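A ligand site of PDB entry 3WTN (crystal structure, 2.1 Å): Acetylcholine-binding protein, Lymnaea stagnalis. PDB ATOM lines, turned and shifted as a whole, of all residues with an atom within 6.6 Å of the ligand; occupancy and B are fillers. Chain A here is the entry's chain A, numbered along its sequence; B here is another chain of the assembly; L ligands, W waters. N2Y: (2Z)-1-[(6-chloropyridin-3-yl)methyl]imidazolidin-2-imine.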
ATOM      1  N   TYR A  93      -2.201  17.807  13.287  1.00  0.00           N
ATOM      2  CA  TYR A  93      -2.872  18.676  14.251  1.00  0.00           C
ATOM      3  C   TYR A  93      -4.077  18.069  14.954  1.00  0.00           C
ATOM      4  O   TYR A  93      -4.251  18.308  16.145  1.00  0.00           O
ATOM      5  CB  TYR A  93      -3.301  19.969  13.559  1.00  0.00           C
ATOM      6  CG  TYR A  93      -2.187  20.952  13.357  1.00  0.00           C
ATOM      7  CD1 TYR A  93      -2.091  22.094  14.162  1.00  0.00           C
ATOM      8  CD2 TYR A  93      -1.205  20.749  12.380  1.00  0.00           C
ATOM      9  CE1 TYR A  93      -1.072  23.010  13.986  1.00  0.00           C
ATOM     10  CE2 TYR A  93      -0.165  21.662  12.214  1.00  0.00           C
ATOM     11  CZ  TYR A  93      -0.108  22.784  13.017  1.00  0.00           C
ATOM     12  OH  TYR A  93       0.889  23.720  12.844  1.00  0.00           O
ATOM     13  N   LYS A 143      -5.138  17.538   9.025  1.00  0.00           N
ATOM     14  CA  LYS A 143      -4.211  18.655   8.878  1.00  0.00           C
ATOM     15  C   LYS A 143      -2.816  18.262   9.333  1.00  0.00           C
ATOM     16  O   LYS A 143      -2.608  17.853  10.476  1.00  0.00           O
ATOM     17  CB  LYS A 143      -4.733  19.858   9.679  1.00  0.00           C
ATOM     18  CG  LYS A 143      -3.775  21.040   9.757  1.00  0.00           C
ATOM     19  CD  LYS A 143      -4.371  22.144  10.634  1.00  0.00           C
ATOM     20  CE  LYS A 143      -3.340  23.196  11.002  1.00  0.00           C
ATOM     21  NZ  LYS A 143      -3.921  24.266  11.878  1.00  0.00           N
ATOM     22  N   GLY A 145       1.421  19.518   9.169  1.00  0.00           N
ATOM     23  CA  GLY A 145       2.397  20.534   8.868  1.00  0.00           C
ATOM     24  C   GLY A 145       3.582  20.441   9.807  1.00  0.00           C
ATOM     25  O   GLY A 145       3.571  19.637  10.753  1.00  0.00           O
ATOM     26  N   SER A 146       4.614  21.248   9.560  1.00  0.00           N
ATOM     27  CA  SER A 146       5.792  21.252  10.421  1.00  0.00           C
ATOM     28  C   SER A 146       5.401  21.843  11.759  1.00  0.00           C
ATOM     29  O   SER A 146       4.683  22.842  11.804  1.00  0.00           O
ATOM     30  CB  SER A 146       6.912  22.105   9.806  1.00  0.00           C
ATOM     31  OG  SER A 146       7.926  22.351  10.754  1.00  0.00           O
ATOM     32  N   TRP A 147       5.854  21.243  12.853  1.00  0.00           N
ATOM     33  CA  TRP A 147       5.476  21.760  14.158  1.00  0.00           C
ATOM     34  C   TRP A 147       6.284  22.967  14.611  1.00  0.00           C
ATOM     35  O   TRP A 147       5.703  23.921  15.121  1.00  0.00           O
ATOM     36  CB  TRP A 147       5.566  20.663  15.232  1.00  0.00           C
ATOM     37  CG  TRP A 147       4.880  21.007  16.525  1.00  0.00           C
ATOM     38  CD1 TRP A 147       5.475  21.249  17.729  1.00  0.00           C
ATOM     39  CD2 TRP A 147       3.469  21.160  16.730  1.00  0.00           C
ATOM     40  NE1 TRP A 147       4.513  21.537  18.683  1.00  0.00           N
ATOM     41  CE2 TRP A 147       3.277  21.478  18.095  1.00  0.00           C
ATOM     42  CE3 TRP A 147       2.344  21.046  15.910  1.00  0.00           C
ATOM     43  CZ2 TRP A 147       2.007  21.699  18.651  1.00  0.00           C
ATOM     44  CZ3 TRP A 147       1.075  21.259  16.460  1.00  0.00           C
ATOM     45  CH2 TRP A 147       0.924  21.576  17.823  1.00  0.00           C
ATOM     46  N   THR A 148       7.594  22.946  14.407  1.00  0.00           N
ATOM     47  CA  THR A 148       8.437  24.052  14.869  1.00  0.00           C
ATOM     48  C   THR A 148       9.128  24.916  13.817  1.00  0.00           C
ATOM     49  O   THR A 148       9.810  25.869  14.166  1.00  0.00           O
ATOM     50  CB  THR A 148       9.535  23.544  15.858  1.00  0.00           C
ATOM     51  OG1 THR A 148      10.591  22.888  15.125  1.00  0.00           O
ATOM     52  CG2 THR A 148       8.928  22.552  16.848  1.00  0.00           C
ATOM     53  N   HIS A 149       8.958  24.597  12.534  1.00  0.00           N
ATOM     54  CA  HIS A 149       9.573  25.376  11.457  1.00  0.00           C
ATOM     55  C   HIS A 149       8.514  26.172  10.687  1.00  0.00           C
ATOM     56  O   HIS A 149       7.561  25.590  10.160  1.00  0.00           O
ATOM     57  CB  HIS A 149      10.314  24.451  10.487  1.00  0.00           C
ATOM     58  CG  HIS A 149      11.504  23.765  11.099  1.00  0.00           C
ATOM     59  ND1 HIS A 149      12.667  24.443  11.393  1.00  0.00           N
ATOM     60  CD2 HIS A 149      11.694  22.485  11.491  1.00  0.00           C
ATOM     61  CE1 HIS A 149      13.532  23.596  11.926  1.00  0.00           C
ATOM     62  NE2 HIS A 149      12.967  22.408  12.000  1.00  0.00           N
ATOM     63  N   TYR A 189      -0.273  31.264  14.463  1.00  0.00           N
ATOM     64  CA  TYR A 189      -0.866  30.898  15.742  1.00  0.00           C
ATOM     65  C   TYR A 189      -0.621  31.972  16.794  1.00  0.00           C
ATOM     66  O   TYR A 189       0.399  32.656  16.756  1.00  0.00           O
ATOM     67  CB  TYR A 189      -0.335  29.535  16.202  1.00  0.00           C
ATOM     68  CG  TYR A 189      -0.654  28.452  15.207  1.00  0.00           C
ATOM     69  CD1 TYR A 189       0.129  28.257  14.064  1.00  0.00           C
ATOM     70  CD2 TYR A 189      -1.834  27.700  15.323  1.00  0.00           C
ATOM     71  CE1 TYR A 189      -0.239  27.363  13.075  1.00  0.00           C
ATOM     72  CE2 TYR A 189      -2.220  26.790  14.334  1.00  0.00           C
ATOM     73  CZ  TYR A 189      -1.424  26.635  13.209  1.00  0.00           C
ATOM     74  OH  TYR A 189      -1.816  25.772  12.206  1.00  0.00           O
ATOM     75  N   CYS A 191       0.485  31.932  19.610  1.00  0.00           N
ATOM     76  CA  CYS A 191       1.746  31.793  20.348  1.00  0.00           C
ATOM     77  C   CYS A 191       2.904  32.473  19.701  1.00  0.00           C
ATOM     78  O   CYS A 191       3.830  32.948  20.360  1.00  0.00           O
ATOM     79  CB  CYS A 191       2.183  30.336  20.437  1.00  0.00           C
ATOM     80  SG  CYS A 191       2.892  29.571  18.899  1.00  0.00           S
ATOM     81  N   CYS A 192       2.853  32.475  18.383  1.00  0.00           N
ATOM     82  CA  CYS A 192       3.992  32.919  17.657  1.00  0.00           C
ATOM     83  C   CYS A 192       3.728  33.865  16.497  1.00  0.00           C
ATOM     84  O   CYS A 192       2.649  33.847  15.900  1.00  0.00           O
ATOM     85  CB  CYS A 192       4.657  31.620  17.221  1.00  0.00           C
ATOM     86  SG  CYS A 192       4.752  30.335  18.541  1.00  0.00           S
ATOM     87  N   TYR A 196       2.858  29.182   9.853  1.00  0.00           N
ATOM     88  CA  TYR A 196       3.258  27.785   9.687  1.00  0.00           C
ATOM     89  C   TYR A 196       2.361  27.158   8.634  1.00  0.00           C
ATOM     90  O   TYR A 196       1.147  27.319   8.666  1.00  0.00           O
ATOM     91  CB  TYR A 196       3.137  27.013  11.011  1.00  0.00           C
ATOM     92  CG  TYR A 196       4.069  27.532  12.081  1.00  0.00           C
ATOM     93  CD1 TYR A 196       3.783  28.716  12.774  1.00  0.00           C
ATOM     94  CD2 TYR A 196       5.283  26.907  12.337  1.00  0.00           C
ATOM     95  CE1 TYR A 196       4.675  29.258  13.686  1.00  0.00           C
ATOM     96  CE2 TYR A 196       6.197  27.438  13.253  1.00  0.00           C
ATOM     97  CZ  TYR A 196       5.884  28.614  13.916  1.00  0.00           C
ATOM     98  OH  TYR A 196       6.788  29.174  14.791  1.00  0.00           O
ATOM     99  N   TRP B  57      -2.184  21.976  24.169  1.00  0.00           N
ATOM    100  CA  TRP B  57      -0.839  22.424  23.845  1.00  0.00           C
ATOM    101  C   TRP B  57      -0.356  23.019  25.157  1.00  0.00           C
ATOM    102  O   TRP B  57      -1.039  23.848  25.751  1.00  0.00           O
ATOM    103  CB  TRP B  57      -0.838  23.518  22.767  1.00  0.00           C
ATOM    104  CG  TRP B  57      -1.296  23.046  21.436  1.00  0.00           C
ATOM    105  CD1 TRP B  57      -1.427  21.749  21.041  1.00  0.00           C
ATOM    106  CD2 TRP B  57      -1.666  23.856  20.324  1.00  0.00           C
ATOM    107  NE1 TRP B  57      -1.869  21.708  19.735  1.00  0.00           N
ATOM    108  CE2 TRP B  57      -2.022  22.984  19.277  1.00  0.00           C
ATOM    109  CE3 TRP B  57      -1.736  25.243  20.112  1.00  0.00           C
ATOM    110  CZ2 TRP B  57      -2.440  23.449  18.017  1.00  0.00           C
ATOM    111  CZ3 TRP B  57      -2.164  25.700  18.859  1.00  0.00           C
ATOM    112  CH2 TRP B  57      -2.510  24.812  17.837  1.00  0.00           C
ATOM    113  N   SER B  79      15.570  24.996  15.910  1.00  0.00           N
ATOM    114  CA  SER B  79      14.715  24.028  16.583  1.00  0.00           C
ATOM    115  C   SER B  79      15.698  23.019  17.193  1.00  0.00           C
ATOM    116  O   SER B  79      16.594  22.529  16.501  1.00  0.00           O
ATOM    117  CB  SER B  79      13.767  23.353  15.596  1.00  0.00           C
ATOM    118  OG  SER B  79      12.770  24.276  15.161  1.00  0.00           O
ATOM    119  N   LEU B 106      10.691  18.919  20.070  1.00  0.00           N
ATOM    120  CA  LEU B 106      11.660  19.942  19.725  1.00  0.00           C
ATOM    121  C   LEU B 106      11.257  21.238  20.405  1.00  0.00           C
ATOM    122  O   LEU B 106      10.086  21.563  20.486  1.00  0.00           O
ATOM    123  CB  LEU B 106      11.666  20.160  18.207  1.00  0.00           C
ATOM    124  CG  LEU B 106      12.014  18.957  17.322  1.00  0.00           C
ATOM    125  CD1 LEU B 106      11.832  19.318  15.865  1.00  0.00           C
ATOM    126  CD2 LEU B 106      13.450  18.531  17.599  1.00  0.00           C
ATOM    127  N   ALA B 107      12.252  21.965  20.904  1.00  0.00           N
ATOM    128  CA  ALA B 107      12.028  23.249  21.534  1.00  0.00           C
ATOM    129  C   ALA B 107      12.564  24.251  20.527  1.00  0.00           C
ATOM    130  O   ALA B 107      13.328  23.887  19.632  1.00  0.00           O
ATOM    131  CB  ALA B 107      12.828  23.350  22.828  1.00  0.00           C
ATOM    132  N   ARG B 108      12.157  25.511  20.652  1.00  0.00           N
ATOM    133  CA  ARG B 108      12.646  26.552  19.764  1.00  0.00           C
ATOM    134  C   ARG B 108      13.542  27.460  20.615  1.00  0.00           C
ATOM    135  O   ARG B 108      13.095  28.006  21.630  1.00  0.00           O
ATOM    136  CB  ARG B 108      11.480  27.338  19.177  1.00  0.00           C
ATOM    137  CG  ARG B 108      11.869  28.292  18.074  1.00  0.00           C
ATOM    138  CD  ARG B 108      12.276  27.572  16.776  1.00  0.00           C
ATOM    139  NE  ARG B 108      12.525  28.550  15.719  1.00  0.00           N
ATOM    140  CZ  ARG B 108      12.845  28.264  14.464  1.00  0.00           C
ATOM    141  NH1 ARG B 108      12.964  27.005  14.055  1.00  0.00           N
ATOM    142  NH2 ARG B 108      13.045  29.249  13.601  1.00  0.00           N
ATOM    143  N   VAL B 109      14.806  27.594  20.229  1.00  0.00           N
ATOM    144  CA  VAL B 109      15.754  28.428  20.959  1.00  0.00           C
ATOM    145  C   VAL B 109      16.082  29.683  20.162  1.00  0.00           C
ATOM    146  O   VAL B 109      16.425  29.605  18.977  1.00  0.00           O
ATOM    147  CB  VAL B 109      17.067  27.656  21.252  1.00  0.00           C
ATOM    148  CG1 VAL B 109      18.010  28.524  22.085  1.00  0.00           C
ATOM    149  CG2 VAL B 109      16.754  26.341  21.979  1.00  0.00           C
ATOM    150  N   LEU B 116      11.234  28.167  23.849  1.00  0.00           N
ATOM    151  CA  LEU B 116       9.825  27.837  23.799  1.00  0.00           C
ATOM    152  C   LEU B 116       9.683  26.350  23.499  1.00  0.00           C
ATOM    153  O   LEU B 116      10.309  25.828  22.587  1.00  0.00           O
ATOM    154  CB  LEU B 116       9.087  28.591  22.690  1.00  0.00           C
ATOM    155  CG  LEU B 116       7.669  28.042  22.424  1.00  0.00           C
ATOM    156  CD1 LEU B 116       6.746  28.322  23.634  1.00  0.00           C
ATOM    157  CD2 LEU B 116       7.073  28.680  21.173  1.00  0.00           C
ATOM    158  N   TYR B 117       8.885  25.674  24.306  1.00  0.00           N
ATOM    159  CA  TYR B 117       8.634  24.262  24.078  1.00  0.00           C
ATOM    160  C   TYR B 117       7.125  24.166  24.196  1.00  0.00           C
ATOM    161  O   TYR B 117       6.549  24.563  25.200  1.00  0.00           O
ATOM    162  CB  TYR B 117       9.321  23.400  25.130  1.00  0.00           C
ATOM    163  CG  TYR B 117       9.001  21.925  24.981  1.00  0.00           C
ATOM    164  CD1 TYR B 117       9.043  21.307  23.730  1.00  0.00           C
ATOM    165  CD2 TYR B 117       8.655  21.157  26.087  1.00  0.00           C
ATOM    166  CE1 TYR B 117       8.735  19.957  23.587  1.00  0.00           C
ATOM    167  CE2 TYR B 117       8.355  19.810  25.959  1.00  0.00           C
ATOM    168  CZ  TYR B 117       8.394  19.214  24.712  1.00  0.00           C
ATOM    169  OH  TYR B 117       8.080  17.887  24.588  1.00  0.00           O
ATOM    170  N   MET B 118       6.484  23.659  23.142  1.00  0.00           N
ATOM    171  CA  MET B 118       5.033  23.584  23.149  1.00  0.00           C
ATOM    172  C   MET B 118       4.493  22.286  22.573  1.00  0.00           C
ATOM    173  O   MET B 118       3.952  22.244  21.457  1.00  0.00           O
ATOM    174  CB  MET B 118       4.451  24.784  22.402  1.00  0.00           C
ATOM    175  CG  MET B 118       2.930  24.860  22.375  1.00  0.00           C
ATOM    176  SD  MET B 118       2.315  26.438  21.727  1.00  0.00           S
ATOM    177  CE  MET B 118       3.709  26.996  20.807  1.00  0.00           C
ATOM    178  N   PRO B 119       4.633  21.187  23.330  1.00  0.00           N
ATOM    179  CA  PRO B 119       4.145  19.907  22.829  1.00  0.00           C
ATOM    180  C   PRO B 119       2.636  19.816  22.939  1.00  0.00           C
ATOM    181  O   PRO B 119       2.005  20.479  23.782  1.00  0.00           O
ATOM    182  CB  PRO B 119       4.821  18.911  23.768  1.00  0.00           C
ATOM    183  CG  PRO B 119       4.776  19.646  25.083  1.00  0.00           C
ATOM    184  CD  PRO B 119       5.186  21.056  24.691  1.00  0.00           C
HETATM  185  N2  N2Y L   1       2.882  24.580  14.418  1.00  0.00           N
HETATM  186  N3  N2Y L   1       3.009  25.859  16.421  1.00  0.00           N
HETATM  187  C1  N2Y L   1       2.381  24.957  15.519  1.00  0.00           C
HETATM  188  N4  N2Y L   1       1.136  24.541  16.030  1.00  0.00           N
HETATM  189  C2  N2Y L   1       0.895  25.180  17.313  1.00  0.00           C
HETATM  190  C3  N2Y L   1       2.123  26.057  17.581  1.00  0.00           C
HETATM  191  C4  N2Y L   1       7.483  25.519  19.059  1.00  0.00           C
HETATM  192 CL1  N2Y L   1       8.739  25.101  20.176  1.00  0.00          CL
HETATM  193  N6  N2Y L   1       6.448  24.663  18.867  1.00  0.00           N
HETATM  194  C5  N2Y L   1       5.451  24.943  18.004  1.00  0.00           C
HETATM  195  C6  N2Y L   1       5.444  26.168  17.253  1.00  0.00           C
HETATM  196  C7  N2Y L   1       6.524  27.066  17.452  1.00  0.00           C
HETATM  197  C8  N2Y L   1       7.562  26.748  18.360  1.00  0.00           C
HETATM  198  C9  N2Y L   1       4.316  26.528  16.265  1.00  0.00           C
HETATM  199  O   HOH W   1       7.317  22.215  20.556  1.00  0.00           O
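OH of Tyr 93 is in hydrogen-bond range of N2 of the ligand (2.7 Å). O of Trp 147 is in hydrogen-bond range of N2 of the ligand.
OH of Tyr 189 sits close to OH of Tyr 93 (3.5 Å). N of Tyr 93 lies within hydrogen-bond range of O of Lys 143 (2.8 Å). O of Leu 116 of chain B sits at hydrogen-bond distance from N of Arg 108 of chain B (2.7 Å). The indole nitrogen (NE1) of Trp 147 sits at hydrogen-bond distance from the backbone carbonyl oxygen (O) of Met 118 of chain B. OG of Ser 79 of chain B is in hydrogen-bond range of NH1 of Arg 108 of chain B. N of His 149 sits at hydrogen-bond distance from OG of Ser 146 (3.0 Å). The side-chain sulfur of Cys 192 forms a disulfide with the side-chain sulfur of Cys 191, 2.0 Å away. The side-chain hydroxyl (OG) of Ser 79 of chain B is in hydrogen-bond range of the side-chain hydroxyl (OG1) of Thr 148, at 2.6 Å.
Ser 146 touches the ligand. Thr 148 touches the ligand (CG2 to N6, 3.8 Å). SG of Cys 191 touches C3 of the ligand, 3.8 Å away. SG of Cys 192 touches C7 of the ligand (3.9 Å). OH of Tyr 196 touches C7 of the ligand, 3.4 Å away. CH2 of Trp 57 of chain B touches C2 of the ligand, at 3.5 Å. Leu 106 of chain B touches the ligand (O to CL1, 3.8 Å). Ala 107 of chain B touches the ligand (C to CL1, 3.9 Å). N of Arg 108 of chain B touches CL1 of the ligand, at 3.5 Å. O of Leu 116 of chain B touches CL1 of the ligand, 3.0 Å away. Tyr 117 of chain B touches the ligand. Met 118 of chain B touches the ligand. Hydrophobic or aromatic side chains within 4 Å of the ligand: Tyr 93, Trp 147, Tyr 196, Trp 57 of chain B, Leu 116 of chain B and Met 118 of chain B. Of the 21 residues printed, 14 come within 4 Å of the ligand. The nearest printed residue that does not touch the ligand is Tyr 189 (4.2 Å).
Water W1 lies within hydrogen-bond range of the backbone carbonyl oxygen (O) of Leu 106 of chain B (2.8 Å), the backbone NH (N) of Met 118 of chain B (3.1 Å), a nitrogen (N6) of the ligand (3.1 Å) and the indole nitrogen (NE1) of Trp 147 (3.4 Å).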
